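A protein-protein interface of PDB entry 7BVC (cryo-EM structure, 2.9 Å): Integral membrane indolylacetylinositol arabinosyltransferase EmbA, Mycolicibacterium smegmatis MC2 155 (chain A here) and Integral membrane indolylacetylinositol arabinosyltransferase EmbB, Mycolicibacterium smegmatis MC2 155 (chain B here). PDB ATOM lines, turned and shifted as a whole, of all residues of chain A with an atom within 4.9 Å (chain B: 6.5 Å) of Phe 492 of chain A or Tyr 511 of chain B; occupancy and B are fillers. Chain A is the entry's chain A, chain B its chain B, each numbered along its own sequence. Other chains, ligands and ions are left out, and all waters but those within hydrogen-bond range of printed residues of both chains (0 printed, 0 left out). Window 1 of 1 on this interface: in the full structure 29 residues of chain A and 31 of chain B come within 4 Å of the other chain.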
ATOM      1  N   GLN A 490      -9.911  -4.421   8.202  1.00  0.00           N
ATOM      2  CA  GLN A 490      -9.566  -4.436   6.783  1.00  0.00           C
ATOM      3  C   GLN A 490      -9.488  -5.875   6.275  1.00  0.00           C
ATOM      4  O   GLN A 490      -8.481  -6.325   5.732  1.00  0.00           O
ATOM      5  CB  GLN A 490      -8.255  -3.689   6.553  1.00  0.00           C
ATOM      6  CG  GLN A 490      -8.306  -2.236   6.985  1.00  0.00           C
ATOM      7  CD  GLN A 490      -7.021  -1.495   6.695  1.00  0.00           C
ATOM      8  OE1 GLN A 490      -6.965  -0.271   6.780  1.00  0.00           O
ATOM      9  NE2 GLN A 490      -5.977  -2.237   6.350  1.00  0.00           N
ATOM     10  N   GLU A 491     -10.591  -6.600   6.466  1.00  0.00           N
ATOM     11  CA  GLU A 491     -10.658  -8.004   6.086  1.00  0.00           C
ATOM     12  C   GLU A 491     -11.070  -8.191   4.632  1.00  0.00           C
ATOM     13  O   GLU A 491     -10.620  -9.145   3.987  1.00  0.00           O
ATOM     14  CB  GLU A 491     -11.627  -8.752   7.004  1.00  0.00           C
ATOM     15  CG  GLU A 491     -11.463 -10.265   7.002  1.00  0.00           C
ATOM     16  CD  GLU A 491     -12.191 -10.945   5.866  1.00  0.00           C
ATOM     17  OE1 GLU A 491     -13.195 -10.384   5.383  1.00  0.00           O
ATOM     18  OE2 GLU A 491     -11.761 -12.046   5.459  1.00  0.00           O
ATOM     19  N   PHE A 492     -11.919  -7.302   4.106  1.00  0.00           N
ATOM     20  CA  PHE A 492     -12.259  -7.306   2.689  1.00  0.00           C
ATOM     21  C   PHE A 492     -11.039  -7.099   1.801  1.00  0.00           C
ATOM     22  O   PHE A 492     -11.125  -7.316   0.583  1.00  0.00           O
ATOM     23  CB  PHE A 492     -13.309  -6.225   2.415  1.00  0.00           C
ATOM     24  CG  PHE A 492     -13.737  -6.140   0.980  1.00  0.00           C
ATOM     25  CD1 PHE A 492     -14.645  -7.043   0.459  1.00  0.00           C
ATOM     26  CD2 PHE A 492     -13.229  -5.153   0.151  1.00  0.00           C
ATOM     27  CE1 PHE A 492     -15.037  -6.966  -0.863  1.00  0.00           C
ATOM     28  CE2 PHE A 492     -13.618  -5.074  -1.170  1.00  0.00           C
ATOM     29  CZ  PHE A 492     -14.523  -5.980  -1.678  1.00  0.00           C
ATOM     30  N   LEU A 493      -9.910  -6.689   2.379  1.00  0.00           N
ATOM     31  CA  LEU A 493      -8.691  -6.518   1.603  1.00  0.00           C
ATOM     32  C   LEU A 493      -8.257  -7.829   0.962  1.00  0.00           C
ATOM     33  O   LEU A 493      -7.623  -7.822  -0.097  1.00  0.00           O
ATOM     34  CB  LEU A 493      -7.594  -5.955   2.506  1.00  0.00           C
ATOM     35  CG  LEU A 493      -6.303  -5.487   1.848  1.00  0.00           C
ATOM     36  CD1 LEU A 493      -6.593  -4.338   0.904  1.00  0.00           C
ATOM     37  CD2 LEU A 493      -5.304  -5.069   2.907  1.00  0.00           C
ATOM     38  N   ARG A 494      -8.625  -8.962   1.564  1.00  0.00           N
ATOM     39  CA  ARG A 494      -8.330 -10.260   0.968  1.00  0.00           C
ATOM     40  C   ARG A 494      -9.092 -10.455  -0.339  1.00  0.00           C
ATOM     41  O   ARG A 494      -8.499 -10.782  -1.376  1.00  0.00           O
ATOM     42  CB  ARG A 494      -8.678 -11.372   1.959  1.00  0.00           C
ATOM     43  CG  ARG A 494      -8.102 -12.725   1.609  1.00  0.00           C
ATOM     44  CD  ARG A 494      -8.532 -13.776   2.618  1.00  0.00           C
ATOM     45  NE  ARG A 494      -7.431 -14.205   3.473  1.00  0.00           N
ATOM     46  CZ  ARG A 494      -7.368 -13.971   4.778  1.00  0.00           C
ATOM     47  NH1 ARG A 494      -6.329 -14.397   5.480  1.00  0.00           N
ATOM     48  NH2 ARG A 494      -8.346 -13.313   5.382  1.00  0.00           N
ATOM     49  N   TYR A 495     -10.411 -10.253  -0.309  1.00  0.00           N
ATOM     50  CA  TYR A 495     -11.216 -10.392  -1.515  1.00  0.00           C
ATOM     51  C   TYR A 495     -10.914  -9.303  -2.531  1.00  0.00           C
ATOM     52  O   TYR A 495     -11.242  -9.463  -3.710  1.00  0.00           O
ATOM     53  CB  TYR A 495     -12.702 -10.381  -1.164  1.00  0.00           C
ATOM     54  CG  TYR A 495     -13.101 -11.477  -0.206  1.00  0.00           C
ATOM     55  CD1 TYR A 495     -13.013 -11.292   1.166  1.00  0.00           C
ATOM     56  CD2 TYR A 495     -13.557 -12.699  -0.674  1.00  0.00           C
ATOM     57  CE1 TYR A 495     -13.369 -12.292   2.043  1.00  0.00           C
ATOM     58  CE2 TYR A 495     -13.916 -13.706   0.197  1.00  0.00           C
ATOM     59  CZ  TYR A 495     -13.821 -13.497   1.553  1.00  0.00           C
ATOM     60  OH  TYR A 495     -14.178 -14.497   2.425  1.00  0.00           O
ATOM     61  N   TYR A 496     -10.307  -8.198  -2.100  1.00  0.00           N
ATOM     62  CA  TYR A 496      -9.826  -7.219  -3.067  1.00  0.00           C
ATOM     63  C   TYR A 496      -8.533  -7.685  -3.725  1.00  0.00           C
ATOM     64  O   TYR A 496      -8.349  -7.510  -4.934  1.00  0.00           O
ATOM     65  CB  TYR A 496      -9.622  -5.862  -2.402  1.00  0.00           C
ATOM     66  CG  TYR A 496      -8.884  -4.879  -3.277  1.00  0.00           C
ATOM     67  CD1 TYR A 496      -9.473  -4.367  -4.423  1.00  0.00           C
ATOM     68  CD2 TYR A 496      -7.598  -4.466  -2.962  1.00  0.00           C
ATOM     69  CE1 TYR A 496      -8.804  -3.472  -5.230  1.00  0.00           C
ATOM     70  CE2 TYR A 496      -6.920  -3.571  -3.762  1.00  0.00           C
ATOM     71  CZ  TYR A 496      -7.529  -3.076  -4.895  1.00  0.00           C
ATOM     72  OH  TYR A 496      -6.860  -2.182  -5.697  1.00  0.00           O
ATOM     73  N   GLU B 507     -15.324  -3.112 -10.222  1.00  0.00           N
ATOM     74  CA  GLU B 507     -16.338  -2.684  -9.267  1.00  0.00           C
ATOM     75  C   GLU B 507     -15.811  -2.679  -7.837  1.00  0.00           C
ATOM     76  O   GLU B 507     -16.235  -1.847  -7.027  1.00  0.00           O
ATOM     77  CB  GLU B 507     -17.566  -3.589  -9.380  1.00  0.00           C
ATOM     78  CG  GLU B 507     -18.607  -3.394  -8.292  1.00  0.00           C
ATOM     79  CD  GLU B 507     -19.250  -2.023  -8.339  1.00  0.00           C
ATOM     80  OE1 GLU B 507     -19.371  -1.462  -9.446  1.00  0.00           O
ATOM     81  OE2 GLU B 507     -19.634  -1.507  -7.270  1.00  0.00           O
ATOM     82  N   ASN B 508     -14.878  -3.577  -7.512  1.00  0.00           N
ATOM     83  CA  ASN B 508     -14.405  -3.715  -6.140  1.00  0.00           C
ATOM     84  C   ASN B 508     -13.667  -2.484  -5.626  1.00  0.00           C
ATOM     85  O   ASN B 508     -13.393  -2.411  -4.425  1.00  0.00           O
ATOM     86  CB  ASN B 508     -13.502  -4.945  -6.017  1.00  0.00           C
ATOM     87  CG  ASN B 508     -12.546  -5.086  -7.183  1.00  0.00           C
ATOM     88  OD1 ASN B 508     -12.052  -4.097  -7.721  1.00  0.00           O
ATOM     89  ND2 ASN B 508     -12.276  -6.323  -7.580  1.00  0.00           N
ATOM     90  N   LEU B 509     -13.345  -1.521  -6.492  1.00  0.00           N
ATOM     91  CA  LEU B 509     -12.690  -0.302  -6.027  1.00  0.00           C
ATOM     92  C   LEU B 509     -13.605   0.504  -5.114  1.00  0.00           C
ATOM     93  O   LEU B 509     -13.141   1.135  -4.155  1.00  0.00           O
ATOM     94  CB  LEU B 509     -12.246   0.545  -7.217  1.00  0.00           C
ATOM     95  CG  LEU B 509     -10.852   0.261  -7.772  1.00  0.00           C
ATOM     96  CD1 LEU B 509     -10.472   1.302  -8.809  1.00  0.00           C
ATOM     97  CD2 LEU B 509      -9.832   0.219  -6.651  1.00  0.00           C
ATOM     98  N   ARG B 510     -14.910   0.499  -5.400  1.00  0.00           N
ATOM     99  CA  ARG B 510     -15.851   1.265  -4.590  1.00  0.00           C
ATOM    100  C   ARG B 510     -15.866   0.791  -3.145  1.00  0.00           C
ATOM    101  O   ARG B 510     -16.064   1.597  -2.230  1.00  0.00           O
ATOM    102  CB  ARG B 510     -17.252   1.177  -5.194  1.00  0.00           C
ATOM    103  CG  ARG B 510     -18.264   2.100  -4.544  1.00  0.00           C
ATOM    104  CD  ARG B 510     -19.629   1.968  -5.190  1.00  0.00           C
ATOM    105  NE  ARG B 510     -19.752   2.792  -6.389  1.00  0.00           N
ATOM    106  CZ  ARG B 510     -19.863   2.303  -7.619  1.00  0.00           C
ATOM    107  NH1 ARG B 510     -19.970   3.125  -8.652  1.00  0.00           N
ATOM    108  NH2 ARG B 510     -19.866   0.994  -7.813  1.00  0.00           N
ATOM    109  N   TYR B 511     -15.661  -0.506  -2.917  1.00  0.00           N
ATOM    110  CA  TYR B 511     -15.592  -1.040  -1.565  1.00  0.00           C
ATOM    111  C   TYR B 511     -14.178  -1.055  -1.009  1.00  0.00           C
ATOM    112  O   TYR B 511     -14.008  -1.083   0.215  1.00  0.00           O
ATOM    113  CB  TYR B 511     -16.172  -2.456  -1.527  1.00  0.00           C
ATOM    114  CG  TYR B 511     -17.526  -2.563  -2.187  1.00  0.00           C
ATOM    115  CD1 TYR B 511     -18.684  -2.261  -1.488  1.00  0.00           C
ATOM    116  CD2 TYR B 511     -17.642  -2.960  -3.510  1.00  0.00           C
ATOM    117  CE1 TYR B 511     -19.921  -2.353  -2.089  1.00  0.00           C
ATOM    118  CE2 TYR B 511     -18.875  -3.055  -4.118  1.00  0.00           C
ATOM    119  CZ  TYR B 511     -20.012  -2.752  -3.404  1.00  0.00           C
ATOM    120  OH  TYR B 511     -21.243  -2.845  -4.006  1.00  0.00           O
ATOM    121  N   TYR B 512     -13.162  -1.042  -1.873  1.00  0.00           N
ATOM    122  CA  TYR B 512     -11.792  -0.907  -1.393  1.00  0.00           C
ATOM    123  C   TYR B 512     -11.529   0.489  -0.846  1.00  0.00           C
ATOM    124  O   TYR B 512     -10.757   0.645   0.105  1.00  0.00           O
ATOM    125  CB  TYR B 512     -10.811  -1.235  -2.518  1.00  0.00           C
ATOM    126  CG  TYR B 512      -9.416  -0.699  -2.305  1.00  0.00           C
ATOM    127  CD1 TYR B 512      -8.595  -1.216  -1.313  1.00  0.00           C
ATOM    128  CD2 TYR B 512      -8.916   0.319  -3.102  1.00  0.00           C
ATOM    129  CE1 TYR B 512      -7.318  -0.730  -1.119  1.00  0.00           C
ATOM    130  CE2 TYR B 512      -7.641   0.810  -2.915  1.00  0.00           C
ATOM    131  CZ  TYR B 512      -6.847   0.282  -1.924  1.00  0.00           C
ATOM    132  OH  TYR B 512      -5.575   0.770  -1.737  1.00  0.00           O
ATOM    133  N   TYR B 513     -12.160   1.512  -1.427  1.00  0.00           N
ATOM    134  CA  TYR B 513     -11.990   2.869  -0.923  1.00  0.00           C
ATOM    135  C   TYR B 513     -12.710   3.093   0.399  1.00  0.00           C
ATOM    136  O   TYR B 513     -12.422   4.074   1.088  1.00  0.00           O
ATOM    137  CB  TYR B 513     -12.492   3.881  -1.952  1.00  0.00           C
ATOM    138  CG  TYR B 513     -11.644   3.975  -3.195  1.00  0.00           C
ATOM    139  CD1 TYR B 513     -10.289   3.688  -3.156  1.00  0.00           C
ATOM    140  CD2 TYR B 513     -12.201   4.354  -4.408  1.00  0.00           C
ATOM    141  CE1 TYR B 513      -9.510   3.773  -4.291  1.00  0.00           C
ATOM    142  CE2 TYR B 513     -11.430   4.442  -5.547  1.00  0.00           C
ATOM    143  CZ  TYR B 513     -10.086   4.150  -5.484  1.00  0.00           C
ATOM    144  OH  TYR B 513      -9.313   4.236  -6.617  1.00  0.00           O
ATOM    145  N   LEU B 514     -13.640   2.210   0.764  1.00  0.00           N
ATOM    146  CA  LEU B 514     -14.437   2.416   1.966  1.00  0.00           C
ATOM    147  C   LEU B 514     -13.723   1.941   3.225  1.00  0.00           C
ATOM    148  O   LEU B 514     -13.964   2.485   4.307  1.00  0.00           O
ATOM    149  CB  LEU B 514     -15.782   1.701   1.826  1.00  0.00           C
ATOM    150  CG  LEU B 514     -16.832   1.962   2.905  1.00  0.00           C
ATOM    151  CD1 LEU B 514     -17.182   3.437   2.961  1.00  0.00           C
ATOM    152  CD2 LEU B 514     -18.072   1.126   2.650  1.00  0.00           C
ATOM    153  N   ILE B 515     -12.842   0.948   3.108  1.00  0.00           N
ATOM    154  CA  ILE B 515     -12.172   0.367   4.264  1.00  0.00           C
ATOM    155  C   ILE B 515     -10.855   1.069   4.575  1.00  0.00           C
ATOM    156  O   ILE B 515     -10.076   0.580   5.397  1.00  0.00           O
ATOM    157  CB  ILE B 515     -11.952  -1.141   4.075  1.00  0.00           C
ATOM    158  CG1 ILE B 515     -10.863  -1.395   3.035  1.00  0.00           C
ATOM    159  CG2 ILE B 515     -13.247  -1.819   3.668  1.00  0.00           C
ATOM    160  CD1 ILE B 515     -10.570  -2.857   2.807  1.00  0.00           C
ATOM    161  N   LEU B 516     -10.593   2.196   3.952  1.00  0.00           N
ATOM    162  CA  LEU B 516      -9.348   2.871   4.269  1.00  0.00           C
ATOM    163  C   LEU B 516      -9.581   3.961   5.308  1.00  0.00           C
ATOM    164  O   LEU B 516     -10.642   4.589   5.331  1.00  0.00           O
ATOM    165  CB  LEU B 516      -8.733   3.490   3.011  1.00  0.00           C
ATOM    166  CG  LEU B 516      -8.475   2.530   1.848  1.00  0.00           C
ATOM    167  CD1 LEU B 516      -7.801   3.253   0.695  1.00  0.00           C
ATOM    168  CD2 LEU B 516      -7.646   1.342   2.301  1.00  0.00           C
ATOM    169  N   PHE B 529     -24.013   2.376   3.997  1.00  0.00           N
ATOM    170  CA  PHE B 529     -23.883   1.047   3.419  1.00  0.00           C
ATOM    171  C   PHE B 529     -23.959  -0.068   4.453  1.00  0.00           C
ATOM    172  O   PHE B 529     -24.565  -1.115   4.182  1.00  0.00           O
ATOM    173  CB  PHE B 529     -22.568   0.927   2.646  1.00  0.00           C
ATOM    174  CG  PHE B 529     -22.426  -0.365   1.902  1.00  0.00           C
ATOM    175  CD1 PHE B 529     -23.270  -0.665   0.849  1.00  0.00           C
ATOM    176  CD2 PHE B 529     -21.453  -1.283   2.257  1.00  0.00           C
ATOM    177  CE1 PHE B 529     -23.147  -1.856   0.162  1.00  0.00           C
ATOM    178  CE2 PHE B 529     -21.325  -2.474   1.575  1.00  0.00           C
ATOM    179  CZ  PHE B 529     -22.174  -2.762   0.525  1.00  0.00           C
ATOM    180  N   MET B 568     -27.686  -2.673  -6.223  1.00  0.00           N
ATOM    181  CA  MET B 568     -26.298  -3.084  -6.030  1.00  0.00           C
ATOM    182  C   MET B 568     -25.712  -3.694  -7.297  1.00  0.00           C
ATOM    183  O   MET B 568     -24.503  -3.602  -7.528  1.00  0.00           O
ATOM    184  CB  MET B 568     -26.191  -4.072  -4.871  1.00  0.00           C
ATOM    185  CG  MET B 568     -25.963  -3.419  -3.522  1.00  0.00           C
ATOM    186  SD  MET B 568     -26.129  -4.586  -2.161  1.00  0.00           S
ATOM    187  CE  MET B 568     -25.286  -6.009  -2.842  1.00  0.00           C
ATOM    188  N   LEU B 571     -25.134  -0.784  -9.899  1.00  0.00           N
ATOM    189  CA  LEU B 571     -24.057   0.127  -9.531  1.00  0.00           C
ATOM    190  C   LEU B 571     -22.766  -0.151 -10.290  1.00  0.00           C
ATOM    191  O   LEU B 571     -21.855   0.681 -10.244  1.00  0.00           O
ATOM    192  CB  LEU B 571     -23.793   0.068  -8.028  1.00  0.00           C
ATOM    193  CG  LEU B 571     -24.484   1.154  -7.201  1.00  0.00           C
ATOM    194  CD1 LEU B 571     -23.981   1.144  -5.768  1.00  0.00           C
ATOM    195  CD2 LEU B 571     -24.289   2.521  -7.836  1.00  0.00           C
ATOM    196  N   ILE B 579     -17.217   6.893  -3.784  1.00  0.00           N
ATOM    197  CA  ILE B 579     -18.001   6.587  -2.594  1.00  0.00           C
ATOM    198  C   ILE B 579     -19.252   7.458  -2.505  1.00  0.00           C
ATOM    199  O   ILE B 579     -20.238   7.048  -1.876  1.00  0.00           O
ATOM    200  CB  ILE B 579     -17.130   6.729  -1.331  1.00  0.00           C
ATOM    201  CG1 ILE B 579     -15.982   5.724  -1.371  1.00  0.00           C
ATOM    202  CG2 ILE B 579     -17.932   6.497  -0.063  1.00  0.00           C
ATOM    203  CD1 ILE B 579     -14.972   5.922  -0.274  1.00  0.00           C
ATOM    204  N   PHE B 582     -22.990   6.202  -2.704  1.00  0.00           N
ATOM    205  CA  PHE B 582     -23.685   5.474  -1.652  1.00  0.00           C
ATOM    206  C   PHE B 582     -24.842   6.263  -1.057  1.00  0.00           C
ATOM    207  O   PHE B 582     -25.577   5.724  -0.226  1.00  0.00           O
ATOM    208  CB  PHE B 582     -22.707   5.082  -0.543  1.00  0.00           C
ATOM    209  CG  PHE B 582     -21.824   3.924  -0.897  1.00  0.00           C
ATOM    210  CD1 PHE B 582     -22.327   2.843  -1.601  1.00  0.00           C
ATOM    211  CD2 PHE B 582     -20.492   3.912  -0.525  1.00  0.00           C
ATOM    212  CE1 PHE B 582     -21.517   1.777  -1.928  1.00  0.00           C
ATOM    213  CE2 PHE B 582     -19.679   2.845  -0.850  1.00  0.00           C
ATOM    214  CZ  PHE B 582     -20.193   1.778  -1.552  1.00  0.00           C
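Printed residues of chain B that touch a printed residue of chain A: Leu 509, Tyr 511, Tyr 512 and Ile 515. Hydrophobic or aromatic side chains of chain B that line the printed part of chain A: Leu 509, Tyr 511, Tyr 512 and Ile 515. Among the printed residues, 5 pairs touch across the chains. Among the printed residues, no Asp or Glu carboxylate lies within 4 Å of a Lys or Arg side-chain nitrogen of the other chain.
Phe 492 of chain A touches just one residue of chain B: Tyr 511. Of the printed residues of chain B, Leu 493 of chain A touches Ile 515 (3.9 Å). Of the printed residues of chain B, Tyr 496 of chain A touches Leu 509 and Tyr 512. Of the printed residues of chain A, Leu 509 of chain B touches Tyr 496. Tyr 511 of chain B touches just one residue of chain A: Phe 492 (3.7 Å). Of the printed residues of chain A, Tyr 512 of chain B touches Tyr 496. Of the printed residues of chain A, Ile 515 of chain B touches Gln 490 (3.5 Å) and Leu 493 (3.9 Å). The nearest residue of chain B that does not touch Phe 492 of chain A is Tyr 512 of chain B (4.1 Å). The nearest printed residue of chain A that does not touch Tyr 511 of chain B is Tyr 496 of chain A (6.7 Å). The nearest printed residue of chain A that does not touch Tyr 512 of chain B is Phe 492 of chain A (4.1 Å).
Among the printed residues, merely in contact across the chains: Gln 490 of chain A with Ile 515 of chain B (3.5 Å), Phe 492 of chain A with Tyr 511 of chain B (3.7 Å), Tyr 496 of chain A with Tyr 512 of chain B (3.8 Å), Leu 493 of chain A with Ile 515 of chain B (3.9 Å) and Tyr 496 of chain A with Leu 509 of chain B (3.9 Å).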
